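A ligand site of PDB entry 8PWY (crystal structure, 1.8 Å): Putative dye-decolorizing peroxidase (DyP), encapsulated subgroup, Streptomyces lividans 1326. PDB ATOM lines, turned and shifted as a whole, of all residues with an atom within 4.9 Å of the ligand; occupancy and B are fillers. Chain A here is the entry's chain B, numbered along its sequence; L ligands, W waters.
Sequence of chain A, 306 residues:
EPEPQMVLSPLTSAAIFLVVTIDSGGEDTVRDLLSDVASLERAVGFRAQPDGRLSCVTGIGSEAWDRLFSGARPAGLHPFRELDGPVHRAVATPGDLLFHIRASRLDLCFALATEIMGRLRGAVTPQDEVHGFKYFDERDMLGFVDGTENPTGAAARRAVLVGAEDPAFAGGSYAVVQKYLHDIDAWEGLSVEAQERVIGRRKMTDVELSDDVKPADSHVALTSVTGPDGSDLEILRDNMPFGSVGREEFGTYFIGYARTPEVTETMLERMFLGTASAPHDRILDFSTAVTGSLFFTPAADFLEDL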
ATOM      1  N   ASP A 140     -29.815  -7.346  33.019  1.00  0.00           N
ATOM      2  CA  ASP A 140     -29.358  -6.236  32.202  1.00  0.00           C
ATOM      3  C   ASP A 140     -30.550  -5.624  31.475  1.00  0.00           C
ATOM      4  O   ASP A 140     -31.692  -6.004  31.703  1.00  0.00           O
ATOM      5  CB  ASP A 140     -28.194  -6.673  31.319  1.00  0.00           C
ATOM      6  CG  ASP A 140     -28.516  -7.730  30.300  1.00  0.00           C
ATOM      7  OD1 ASP A 140     -29.701  -7.841  29.934  1.00  0.00           O
ATOM      8  OD2 ASP A 140     -27.580  -8.425  29.879  1.00  0.00           O
ATOM      9  N   LEU A 142     -31.538  -5.956  28.502  1.00  0.00           N
ATOM     10  CA  LEU A 142     -32.240  -6.884  27.646  1.00  0.00           C
ATOM     11  C   LEU A 142     -33.084  -7.834  28.484  1.00  0.00           C
ATOM     12  O   LEU A 142     -33.803  -8.660  27.926  1.00  0.00           O
ATOM     13  CB  LEU A 142     -31.234  -7.673  26.815  1.00  0.00           C
ATOM     14  CG  LEU A 142     -30.365  -6.842  25.863  1.00  0.00           C
ATOM     15  CD1 LEU A 142     -29.507  -7.722  24.965  1.00  0.00           C
ATOM     16  CD2 LEU A 142     -31.172  -5.924  24.963  1.00  0.00           C
ATOM     17  N   PHE A 144     -32.000 -10.150  30.723  1.00  0.00           N
ATOM     18  CA  PHE A 144     -31.336 -11.420  30.995  1.00  0.00           C
ATOM     19  C   PHE A 144     -30.389 -11.236  32.175  1.00  0.00           C
ATOM     20  O   PHE A 144     -29.812 -10.170  32.338  1.00  0.00           O
ATOM     21  CB  PHE A 144     -30.568 -11.920  29.768  1.00  0.00           C
ATOM     22  CG  PHE A 144     -31.412 -12.625  28.756  1.00  0.00           C
ATOM     23  CD1 PHE A 144     -32.312 -11.945  27.979  1.00  0.00           C
ATOM     24  CD2 PHE A 144     -31.320 -14.008  28.607  1.00  0.00           C
ATOM     25  CE1 PHE A 144     -33.111 -12.610  27.061  1.00  0.00           C
ATOM     26  CE2 PHE A 144     -32.128 -14.688  27.702  1.00  0.00           C
ATOM     27  CZ  PHE A 144     -33.022 -13.988  26.925  1.00  0.00           C
ATOM     28  N   VAL A 145     -30.221 -12.293  32.984  1.00  0.00           N
ATOM     29  CA  VAL A 145     -29.223 -12.288  34.051  1.00  0.00           C
ATOM     30  C   VAL A 145     -27.862 -12.147  33.393  1.00  0.00           C
ATOM     31  O   VAL A 145     -27.576 -12.817  32.391  1.00  0.00           O
ATOM     32  CB  VAL A 145     -29.328 -13.553  34.925  1.00  0.00           C
ATOM     33  CG1 VAL A 145     -28.271 -13.537  36.022  1.00  0.00           C
ATOM     34  CG2 VAL A 145     -30.747 -13.791  35.473  1.00  0.00           C
ATOM     35  N   ASP A 146     -26.993 -11.302  33.980  1.00  0.00           N
ATOM     36  CA  ASP A 146     -25.739 -10.912  33.343  1.00  0.00           C
ATOM     37  C   ASP A 146     -24.639 -11.032  34.386  1.00  0.00           C
ATOM     38  O   ASP A 146     -24.697 -10.358  35.401  1.00  0.00           O
ATOM     39  CB  ASP A 146     -25.907  -9.500  32.781  1.00  0.00           C
ATOM     40  CG  ASP A 146     -24.837  -8.995  31.823  1.00  0.00           C
ATOM     41  OD1 ASP A 146     -23.667  -9.213  32.164  1.00  0.00           O
ATOM     42  OD2 ASP A 146     -25.217  -8.246  30.812  1.00  0.00           O
ATOM     43  N   GLY A 147     -23.694 -11.940  34.167  1.00  0.00           N
ATOM     44  CA  GLY A 147     -22.594 -12.195  35.090  1.00  0.00           C
ATOM     45  C   GLY A 147     -22.437 -13.678  35.492  1.00  0.00           C
ATOM     46  O   GLY A 147     -21.441 -14.054  36.101  1.00  0.00           O
ATOM     47  N   THR A 148     -23.404 -14.519  35.129  1.00  0.00           N
ATOM     48  CA  THR A 148     -23.549 -15.876  35.625  1.00  0.00           C
ATOM     49  C   THR A 148     -22.265 -16.692  35.458  1.00  0.00           C
ATOM     50  O   THR A 148     -21.850 -17.360  36.376  1.00  0.00           O
ATOM     51  CB  THR A 148     -24.681 -16.549  34.864  1.00  0.00           C
ATOM     52  OG1 THR A 148     -25.797 -15.688  34.997  1.00  0.00           O
ATOM     53  CG2 THR A 148     -25.009 -17.903  35.416  1.00  0.00           C
ATOM     54  N   GLU A 149     -21.653 -16.654  34.266  1.00  0.00           N
ATOM     55  CA  GLU A 149     -20.530 -17.553  34.017  1.00  0.00           C
ATOM     56  C   GLU A 149     -19.209 -16.827  34.245  1.00  0.00           C
ATOM     57  O   GLU A 149     -18.163 -17.317  33.846  1.00  0.00           O
ATOM     58  CB  GLU A 149     -20.564 -18.148  32.605  1.00  0.00           C
ATOM     59  CG  GLU A 149     -21.630 -19.223  32.480  1.00  0.00           C
ATOM     60  CD  GLU A 149     -21.468 -20.436  33.392  1.00  0.00           C
ATOM     61  OE1 GLU A 149     -20.437 -21.001  33.319  1.00  0.00           O
ATOM     62  OE2 GLU A 149     -22.345 -20.735  34.167  1.00  0.00           O
ATOM     63  N   ASN A 150     -19.209 -15.675  34.908  1.00  0.00           N
ATOM     64  CA  ASN A 150     -17.925 -15.111  35.291  1.00  0.00           C
ATOM     65  C   ASN A 150     -17.164 -16.124  36.146  1.00  0.00           C
ATOM     66  O   ASN A 150     -17.760 -16.786  36.996  1.00  0.00           O
ATOM     67  CB  ASN A 150     -18.042 -13.846  36.139  1.00  0.00           C
ATOM     68  CG  ASN A 150     -18.114 -12.598  35.316  1.00  0.00           C
ATOM     69  OD1 ASN A 150     -17.493 -12.480  34.263  1.00  0.00           O
ATOM     70  ND2 ASN A 150     -18.853 -11.626  35.792  1.00  0.00           N
ATOM     71  N   GLN A 178     -16.577  -0.924  26.084  1.00  0.00           N
ATOM     72  CA  GLN A 178     -17.408  -0.505  24.974  1.00  0.00           C
ATOM     73  C   GLN A 178     -18.765  -0.044  25.545  1.00  0.00           C
ATOM     74  O   GLN A 178     -19.426  -0.797  26.250  1.00  0.00           O
ATOM     75  CB  GLN A 178     -17.693  -1.661  24.017  1.00  0.00           C
ATOM     76  CG  GLN A 178     -16.517  -2.164  23.231  1.00  0.00           C
ATOM     77  CD  GLN A 178     -16.950  -3.322  22.379  1.00  0.00           C
ATOM     78  OE1 GLN A 178     -17.395  -4.365  22.842  1.00  0.00           O
ATOM     79  NE2 GLN A 178     -16.887  -3.110  21.080  1.00  0.00           N
ATOM     80  N   TYR A 180     -22.544   0.346  24.684  1.00  0.00           N
ATOM     81  CA  TYR A 180     -23.517  -0.157  23.711  1.00  0.00           C
ATOM     82  C   TYR A 180     -24.844   0.543  23.931  1.00  0.00           C
ATOM     83  O   TYR A 180     -25.298   0.655  25.054  1.00  0.00           O
ATOM     84  CB  TYR A 180     -23.731  -1.673  23.790  1.00  0.00           C
ATOM     85  CG  TYR A 180     -22.613  -2.518  23.222  1.00  0.00           C
ATOM     86  CD1 TYR A 180     -22.623  -2.893  21.904  1.00  0.00           C
ATOM     87  CD2 TYR A 180     -21.576  -2.982  24.015  1.00  0.00           C
ATOM     88  CE1 TYR A 180     -21.625  -3.699  21.364  1.00  0.00           C
ATOM     89  CE2 TYR A 180     -20.587  -3.822  23.505  1.00  0.00           C
ATOM     90  CZ  TYR A 180     -20.582  -4.151  22.152  1.00  0.00           C
ATOM     91  OH  TYR A 180     -19.592  -4.940  21.651  1.00  0.00           O
ATOM     92  N   HIS A 182     -28.909   0.035  22.754  1.00  0.00           N
ATOM     93  CA  HIS A 182     -29.742  -1.024  22.288  1.00  0.00           C
ATOM     94  C   HIS A 182     -30.954  -0.457  21.547  1.00  0.00           C
ATOM     95  O   HIS A 182     -31.407   0.621  21.834  1.00  0.00           O
ATOM     96  CB  HIS A 182     -30.238  -1.864  23.456  1.00  0.00           C
ATOM     97  CG  HIS A 182     -29.185  -2.607  24.151  1.00  0.00           C
ATOM     98  ND1 HIS A 182     -28.486  -3.640  23.576  1.00  0.00           N
ATOM     99  CD2 HIS A 182     -28.759  -2.482  25.417  1.00  0.00           C
ATOM    100  CE1 HIS A 182     -27.622  -4.107  24.485  1.00  0.00           C
ATOM    101  NE2 HIS A 182     -27.764  -3.404  25.612  1.00  0.00           N
ATOM    102  N   ILE A 199     -29.274 -15.073  22.909  1.00  0.00           N
ATOM    103  CA  ILE A 199     -28.333 -15.057  24.022  1.00  0.00           C
ATOM    104  C   ILE A 199     -27.683 -16.430  24.181  1.00  0.00           C
ATOM    105  O   ILE A 199     -26.474 -16.515  24.334  1.00  0.00           O
ATOM    106  CB  ILE A 199     -29.065 -14.614  25.315  1.00  0.00           C
ATOM    107  CG1 ILE A 199     -29.664 -13.219  25.188  1.00  0.00           C
ATOM    108  CG2 ILE A 199     -28.142 -14.735  26.520  1.00  0.00           C
ATOM    109  CD1 ILE A 199     -28.666 -12.137  24.947  1.00  0.00           C
ATOM    110  N   ARG A 201     -29.209 -18.714  26.543  1.00  0.00           N
ATOM    111  CA  ARG A 201     -29.640 -19.175  27.858  1.00  0.00           C
ATOM    112  C   ARG A 201     -31.113 -18.911  27.988  1.00  0.00           C
ATOM    113  O   ARG A 201     -31.617 -18.045  27.277  1.00  0.00           O
ATOM    114  CB  ARG A 201     -28.918 -18.434  29.002  1.00  0.00           C
ATOM    115  CG  ARG A 201     -27.412 -18.362  28.850  1.00  0.00           C
ATOM    116  CD  ARG A 201     -26.743 -17.664  30.011  1.00  0.00           C
ATOM    117  NE  ARG A 201     -26.813 -18.396  31.287  1.00  0.00           N
ATOM    118  CZ  ARG A 201     -26.004 -19.385  31.674  1.00  0.00           C
ATOM    119  NH1 ARG A 201     -26.413 -20.220  32.627  1.00  0.00           N
ATOM    120  NH2 ARG A 201     -24.842 -19.631  31.059  1.00  0.00           N
ATOM    121  N   ASP A 206     -32.308 -18.748  33.613  1.00  0.00           N
ATOM    122  CA  ASP A 206     -30.889 -18.558  33.372  1.00  0.00           C
ATOM    123  C   ASP A 206     -30.151 -19.892  33.214  1.00  0.00           C
ATOM    124  O   ASP A 206     -28.952 -19.945  33.397  1.00  0.00           O
ATOM    125  CB  ASP A 206     -30.234 -17.722  34.474  1.00  0.00           C
ATOM    126  CG  ASP A 206     -28.883 -17.110  34.103  1.00  0.00           C
ATOM    127  OD1 ASP A 206     -28.583 -16.961  32.891  1.00  0.00           O
ATOM    128  OD2 ASP A 206     -28.127 -16.784  35.003  1.00  0.00           O
ATOM    129  N   HIS A 219     -24.877 -15.509  21.469  1.00  0.00           N
ATOM    130  CA  HIS A 219     -23.839 -14.748  22.161  1.00  0.00           C
ATOM    131  C   HIS A 219     -22.939 -15.684  22.970  1.00  0.00           C
ATOM    132  O   HIS A 219     -21.708 -15.565  22.953  1.00  0.00           O
ATOM    133  CB  HIS A 219     -24.521 -13.666  23.018  1.00  0.00           C
ATOM    134  CG  HIS A 219     -23.580 -12.844  23.758  1.00  0.00           C
ATOM    135  ND1 HIS A 219     -22.604 -12.118  23.106  1.00  0.00           N
ATOM    136  CD2 HIS A 219     -23.413 -12.646  25.071  1.00  0.00           C
ATOM    137  CE1 HIS A 219     -21.881 -11.462  24.045  1.00  0.00           C
ATOM    138  NE2 HIS A 219     -22.388 -11.744  25.229  1.00  0.00           N
ATOM    139  N   VAL A 220     -23.556 -16.620  23.673  1.00  0.00           N
ATOM    140  CA  VAL A 220     -22.804 -17.551  24.497  1.00  0.00           C
ATOM    141  C   VAL A 220     -21.966 -18.472  23.621  1.00  0.00           C
ATOM    142  O   VAL A 220     -20.848 -18.821  24.028  1.00  0.00           O
ATOM    143  CB  VAL A 220     -23.737 -18.345  25.410  1.00  0.00           C
ATOM    144  CG1 VAL A 220     -23.120 -19.651  25.881  1.00  0.00           C
ATOM    145  CG2 VAL A 220     -24.191 -17.500  26.574  1.00  0.00           C
ATOM    146  N   THR A 223     -18.893 -16.349  22.340  1.00  0.00           N
ATOM    147  CA  THR A 223     -17.937 -15.849  23.327  1.00  0.00           C
ATOM    148  C   THR A 223     -17.361 -16.997  24.152  1.00  0.00           C
ATOM    149  O   THR A 223     -16.666 -16.725  25.119  1.00  0.00           O
ATOM    150  CB  THR A 223     -18.581 -14.797  24.237  1.00  0.00           C
ATOM    151  OG1 THR A 223     -19.749 -15.302  24.906  1.00  0.00           O
ATOM    152  CG2 THR A 223     -18.931 -13.554  23.447  1.00  0.00           C
ATOM    153  N   SER A 224     -17.661 -18.258  23.810  1.00  0.00           N
ATOM    154  CA  SER A 224     -16.981 -19.422  24.386  1.00  0.00           C
ATOM    155  C   SER A 224     -15.777 -19.782  23.516  1.00  0.00           C
ATOM    156  O   SER A 224     -15.938 -20.063  22.337  1.00  0.00           O
ATOM    157  CB  SER A 224     -17.878 -20.591  24.514  1.00  0.00           C
ATOM    158  OG  SER A 224     -18.957 -20.284  25.387  1.00  0.00           O
ATOM    159  N   ILE A 235     -12.800 -14.364  30.756  1.00  0.00           N
ATOM    160  CA  ILE A 235     -12.636 -12.984  31.149  1.00  0.00           C
ATOM    161  C   ILE A 235     -13.583 -12.721  32.300  1.00  0.00           C
ATOM    162  O   ILE A 235     -14.480 -13.514  32.602  1.00  0.00           O
ATOM    163  CB  ILE A 235     -12.894 -12.001  29.991  1.00  0.00           C
ATOM    164  CG1 ILE A 235     -14.349 -11.997  29.555  1.00  0.00           C
ATOM    165  CG2 ILE A 235     -11.972 -12.280  28.835  1.00  0.00           C
ATOM    166  CD1 ILE A 235     -14.606 -10.888  28.537  1.00  0.00           C
ATOM    167  N   ARG A 237     -16.265  -9.915  33.612  1.00  0.00           N
ATOM    168  CA  ARG A 237     -17.098  -8.832  33.122  1.00  0.00           C
ATOM    169  C   ARG A 237     -17.865  -8.198  34.272  1.00  0.00           C
ATOM    170  O   ARG A 237     -18.171  -8.874  35.228  1.00  0.00           O
ATOM    171  CB  ARG A 237     -18.117  -9.336  32.092  1.00  0.00           C
ATOM    172  CG  ARG A 237     -17.495  -9.913  30.838  1.00  0.00           C
ATOM    173  CD  ARG A 237     -18.521 -10.709  30.045  1.00  0.00           C
ATOM    174  NE  ARG A 237     -18.812 -11.964  30.733  1.00  0.00           N
ATOM    175  CZ  ARG A 237     -19.996 -12.348  31.207  1.00  0.00           C
ATOM    176  NH1 ARG A 237     -21.063 -11.639  30.969  1.00  0.00           N
ATOM    177  NH2 ARG A 237     -20.111 -13.489  31.902  1.00  0.00           N
ATOM    178  N   ASN A 239     -20.707  -5.749  33.378  1.00  0.00           N
ATOM    179  CA  ASN A 239     -21.567  -4.953  32.524  1.00  0.00           C
ATOM    180  C   ASN A 239     -22.644  -4.245  33.362  1.00  0.00           C
ATOM    181  O   ASN A 239     -23.232  -4.814  34.274  1.00  0.00           O
ATOM    182  CB  ASN A 239     -22.300  -5.838  31.507  1.00  0.00           C
ATOM    183  CG  ASN A 239     -21.390  -6.563  30.563  1.00  0.00           C
ATOM    184  OD1 ASN A 239     -20.171  -6.278  30.475  1.00  0.00           O
ATOM    185  ND2 ASN A 239     -21.956  -7.597  29.951  1.00  0.00           N
ATOM    186  N   THR A 252     -26.020  -0.785  27.555  1.00  0.00           N
ATOM    187  CA  THR A 252     -25.184  -1.660  28.346  1.00  0.00           C
ATOM    188  C   THR A 252     -23.760  -1.139  28.254  1.00  0.00           C
ATOM    189  O   THR A 252     -23.248  -0.988  27.163  1.00  0.00           O
ATOM    190  CB  THR A 252     -25.235  -3.105  27.887  1.00  0.00           C
ATOM    191  OG1 THR A 252     -26.564  -3.626  28.023  1.00  0.00           O
ATOM    192  CG2 THR A 252     -24.250  -3.975  28.667  1.00  0.00           C
ATOM    193  N   PHE A 254     -20.236  -2.227  28.633  1.00  0.00           N
ATOM    194  CA  PHE A 254     -19.410  -3.418  28.696  1.00  0.00           C
ATOM    195  C   PHE A 254     -18.041  -3.074  29.245  1.00  0.00           C
ATOM    196  O   PHE A 254     -17.381  -2.169  28.771  1.00  0.00           O
ATOM    197  CB  PHE A 254     -19.196  -4.006  27.308  1.00  0.00           C
ATOM    198  CG  PHE A 254     -18.238  -5.166  27.305  1.00  0.00           C
ATOM    199  CD1 PHE A 254     -18.637  -6.421  27.733  1.00  0.00           C
ATOM    200  CD2 PHE A 254     -16.932  -4.963  26.924  1.00  0.00           C
ATOM    201  CE1 PHE A 254     -17.758  -7.490  27.751  1.00  0.00           C
ATOM    202  CE2 PHE A 254     -16.031  -6.013  26.993  1.00  0.00           C
ATOM    203  CZ  PHE A 254     -16.436  -7.263  27.409  1.00  0.00           C
ATOM    204  N   THR A 264      -9.766 -11.224  25.048  1.00  0.00           N
ATOM    205  CA  THR A 264     -10.900 -10.339  24.810  1.00  0.00           C
ATOM    206  C   THR A 264     -11.018 -10.028  23.326  1.00  0.00           C
ATOM    207  O   THR A 264     -12.131 -10.003  22.777  1.00  0.00           O
ATOM    208  CB  THR A 264     -10.787  -9.058  25.643  1.00  0.00           C
ATOM    209  OG1 THR A 264     -10.564  -9.476  26.984  1.00  0.00           O
ATOM    210  CG2 THR A 264     -12.040  -8.233  25.630  1.00  0.00           C
ATOM    211  N   MET A 267     -12.582 -12.864  21.338  1.00  0.00           N
ATOM    212  CA  MET A 267     -14.036 -12.885  21.510  1.00  0.00           C
ATOM    213  C   MET A 267     -14.669 -11.805  20.633  1.00  0.00           C
ATOM    214  O   MET A 267     -15.677 -12.041  19.965  1.00  0.00           O
ATOM    215  CB  MET A 267     -14.382 -12.643  22.975  1.00  0.00           C
ATOM    216  CG  MET A 267     -14.042 -13.838  23.836  1.00  0.00           C
ATOM    217  SD  MET A 267     -14.297 -13.405  25.589  1.00  0.00           S
ATOM    218  CE  MET A 267     -13.891 -14.951  26.396  1.00  0.00           C
ATOM    219  N   LEU A 268     -14.071 -10.601  20.603  1.00  0.00           N
ATOM    220  CA  LEU A 268     -14.619  -9.537  19.783  1.00  0.00           C
ATOM    221  C   LEU A 268     -14.591  -9.882  18.284  1.00  0.00           C
ATOM    222  O   LEU A 268     -15.523  -9.524  17.570  1.00  0.00           O
ATOM    223  CB  LEU A 268     -13.860  -8.258  20.052  1.00  0.00           C
ATOM    224  CG  LEU A 268     -14.245  -7.521  21.335  1.00  0.00           C
ATOM    225  CD1 LEU A 268     -13.285  -6.353  21.562  1.00  0.00           C
ATOM    226  CD2 LEU A 268     -15.655  -6.999  21.288  1.00  0.00           C
ATOM    227  N   MET A 271     -17.387 -12.138  17.503  1.00  0.00           N
ATOM    228  CA  MET A 271     -18.667 -11.471  17.558  1.00  0.00           C
ATOM    229  C   MET A 271     -18.887 -10.625  16.296  1.00  0.00           C
ATOM    230  O   MET A 271     -19.971 -10.623  15.740  1.00  0.00           O
ATOM    231  CB  MET A 271     -18.746 -10.573  18.798  1.00  0.00           C
ATOM    232  CG  MET A 271     -18.920 -11.347  20.080  1.00  0.00           C
ATOM    233  SD  MET A 271     -18.879 -10.139  21.503  1.00  0.00           S
ATOM    234  CE  MET A 271     -20.326  -9.134  21.224  1.00  0.00           C
ATOM    235  N   ILE A 283     -26.510 -10.766  19.070  1.00  0.00           N
ATOM    236  CA  ILE A 283     -26.755  -9.683  20.001  1.00  0.00           C
ATOM    237  C   ILE A 283     -26.470  -8.342  19.343  1.00  0.00           C
ATOM    238  O   ILE A 283     -27.033  -7.324  19.731  1.00  0.00           O
ATOM    239  CB  ILE A 283     -25.982  -9.876  21.319  1.00  0.00           C
ATOM    240  CG1 ILE A 283     -26.752  -9.298  22.494  1.00  0.00           C
ATOM    241  CG2 ILE A 283     -24.550  -9.349  21.210  1.00  0.00           C
ATOM    242  CD1 ILE A 283     -26.106  -9.610  23.850  1.00  0.00           C
ATOM    243  N   SER A 287     -27.698  -4.173  19.276  1.00  0.00           N
ATOM    244  CA  SER A 287     -26.751  -3.473  20.113  1.00  0.00           C
ATOM    245  C   SER A 287     -25.716  -2.800  19.213  1.00  0.00           C
ATOM    246  O   SER A 287     -25.087  -3.498  18.405  1.00  0.00           O
ATOM    247  CB  SER A 287     -26.064  -4.450  21.087  1.00  0.00           C
ATOM    248  OG  SER A 287     -27.006  -5.328  21.697  1.00  0.00           O
HETATM  249  C1  LIG L   1     -22.234 -13.877  28.595  1.00  0.00           C
HETATM  250  C2  LIG L   1     -24.870  -9.927  27.857  1.00  0.00           C
HETATM  251  C3  LIG L   1     -21.259  -7.853  25.330  1.00  0.00           C
HETATM  252  C4  LIG L   1     -18.543 -11.627  26.566  1.00  0.00           C
HETATM  253  C5  LIG L   1     -23.256 -12.930  28.501  1.00  0.00           C
HETATM  254  C6  LIG L   1     -24.559 -13.215  28.992  1.00  0.00           C
HETATM  255  C7  LIG L   1     -25.272 -12.077  28.810  1.00  0.00           C
HETATM  256  C8  LIG L   1     -24.415 -11.144  28.205  1.00  0.00           C
HETATM  257  C9  LIG L   1     -26.713 -11.867  29.179  1.00  0.00           C
HETATM  258  C10 LIG L   1     -25.039 -14.515  29.647  1.00  0.00           C
HETATM  259  C11 LIG L   1     -24.958 -14.550  31.194  1.00  0.00           C
HETATM  260  C12 LIG L   1     -23.480 -14.439  31.636  1.00  0.00           C
HETATM  261  O1  LIG L   1     -22.963 -13.310  31.900  1.00  0.00           O
HETATM  262  O2  LIG L   1     -22.755 -15.519  31.706  1.00  0.00           O
HETATM  263  C13 LIG L   1     -24.118  -9.053  27.123  1.00  0.00           C
HETATM  264  C14 LIG L   1     -24.622  -7.800  26.661  1.00  0.00           C
HETATM  265  C15 LIG L   1     -23.637  -7.164  25.934  1.00  0.00           C
HETATM  266  C16 LIG L   1     -22.496  -8.104  25.945  1.00  0.00           C
HETATM  267  C17 LIG L   1     -26.002  -7.214  26.930  1.00  0.00           C
HETATM  268  C18 LIG L   1     -23.915  -5.881  25.227  1.00  0.00           C
HETATM  269  C19 LIG L   1     -23.639  -5.828  23.967  1.00  0.00           C
HETATM  270  C20 LIG L   1     -20.186  -8.726  25.439  1.00  0.00           C
HETATM  271  C21 LIG L   1     -18.937  -8.553  24.847  1.00  0.00           C
HETATM  272  C22 LIG L   1     -18.156  -9.624  25.178  1.00  0.00           C
HETATM  273  C23 LIG L   1     -18.995 -10.474  25.962  1.00  0.00           C
HETATM  274  C24 LIG L   1     -18.600  -7.363  24.063  1.00  0.00           C
HETATM  275  C25 LIG L   1     -16.695  -9.946  24.905  1.00  0.00           C
HETATM  276  C26 LIG L   1     -15.803  -9.172  24.349  1.00  0.00           C
HETATM  277  C27 LIG L   1     -19.316 -12.543  27.228  1.00  0.00           C
HETATM  278  C28 LIG L   1     -18.738 -13.770  27.756  1.00  0.00           C
HETATM  279  C29 LIG L   1     -19.804 -14.401  28.274  1.00  0.00           C
HETATM  280  C30 LIG L   1     -20.966 -13.533  28.133  1.00  0.00           C
HETATM  281  C31 LIG L   1     -17.325 -14.309  27.717  1.00  0.00           C
HETATM  282  C32 LIG L   1     -19.743 -15.763  28.933  1.00  0.00           C
HETATM  283  C33 LIG L   1     -19.812 -16.972  27.973  1.00  0.00           C
HETATM  284  C34 LIG L   1     -19.798 -18.347  28.629  1.00  0.00           C
HETATM  285  O3  LIG L   1     -20.890 -18.845  29.056  1.00  0.00           O
HETATM  286  O4  LIG L   1     -18.720 -18.973  28.752  1.00  0.00           O
HETATM  287  N1  LIG L   1     -23.195 -11.654  28.018  1.00  0.00           N
HETATM  288  N2  LIG L   1     -22.878  -9.225  26.664  1.00  0.00           N
HETATM  289  N3  LIG L   1     -20.222  -9.915  26.118  1.00  0.00           N
HETATM  290  N4  LIG L   1     -20.641 -12.416  27.444  1.00  0.00           N
HETATM  291 FE1  LIG L   1     -21.711 -10.876  27.026  1.00  0.00          FE
HETATM  292  O   HOH W   1     -16.455 -17.563  27.810  1.00  0.00           O
HETATM  293  O   HOH W   2     -23.125 -17.583  29.812  1.00  0.00           O
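NE2 of His 219 binds FE1 of the ligand. The guanidinium group (NH1) of Arg 237 is in salt-bridge range of an oxygen (O1) of the ligand, at 2.7 Å. N of Gly 147 lies within hydrogen-bond range of O1 of the ligand (2.7 Å). The backbone NH of Glu 149 is in hydrogen-bond range of an oxygen (O2) of the ligand (3.0 Å). The backbone NH (N) of Thr 148 is in hydrogen-bond range of an oxygen (O1) of the ligand (3.5 Å).
Residues that only touch the ligand: Phe 254 (3.3 Å), Val 145 (3.4 Å), Thr 223 (3.4 Å), Asp 146 (3.4 Å), Gln 178 (3.5 Å), Tyr 180 (3.5 Å), Asp 140 (3.6 Å), Arg 201 (3.6 Å), Ser 224 (3.6 Å), Ile 283 (3.7 Å), Met 271 (3.7 Å), Met 267 (3.7 Å), Leu 268 (3.8 Å), Asn 239 (3.8 Å), Thr 252 (3.8 Å), Phe 144 (3.9 Å) and Val 220 (3.96 Å). Hydrophobic or aromatic side chains that line the ligand: Phe 144, Tyr 180, His 219, Val 220, Phe 254, Met 267, Leu 268, Met 271 and Ile 283. Within 4 Å of the ligand: Asp 140, Phe 144, Val 145, Asp 146, Gly 147, Thr 148, Glu 149, Gln 178, Tyr 180, Arg 201, His 219, Val 220, Thr 223, Ser 224, Arg 237, Asn 239, Thr 252, Phe 254, Met 267, Leu 268, Met 271 and Ile 283. The nearest printed residue that does not touch the ligand is Ser 287 (4.01 Å).
Water W2 lies within hydrogen-bond range of an oxygen (O3) of the ligand (2.7 Å) and the guanidinium group of Arg 201 (2.9 Å). Water W1 bridges O of Thr 223 (2.8 Å) and O4 of the ligand (2.8 Å).
O of His 219 is in hydrogen-bond range of OG1 of Thr 223 (2.8 Å). The backbone NH (N) of Phe 254 lies within hydrogen-bond range of the backbone carbonyl oxygen (O) of Gln 178 (2.9 Å). OD1 of Asp 146 sits at hydrogen-bond distance from ND2 of Asn 239 (3.2 Å). N of Tyr 180 sits at hydrogen-bond distance from O of Thr 252. N of Leu 142 is in hydrogen-bond range of OD1 of Asp 140, 3.0 Å away. NE of Arg 201 is in salt-bridge range of OD1 of Asp 206. The side-chain hydroxyl (OG) of Ser 224 is in hydrogen-bond range of the backbone carbonyl oxygen (O) of Val 220. NE2 of His 182 sits at hydrogen-bond distance from OG1 of Thr 252, 2.7 Å away.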
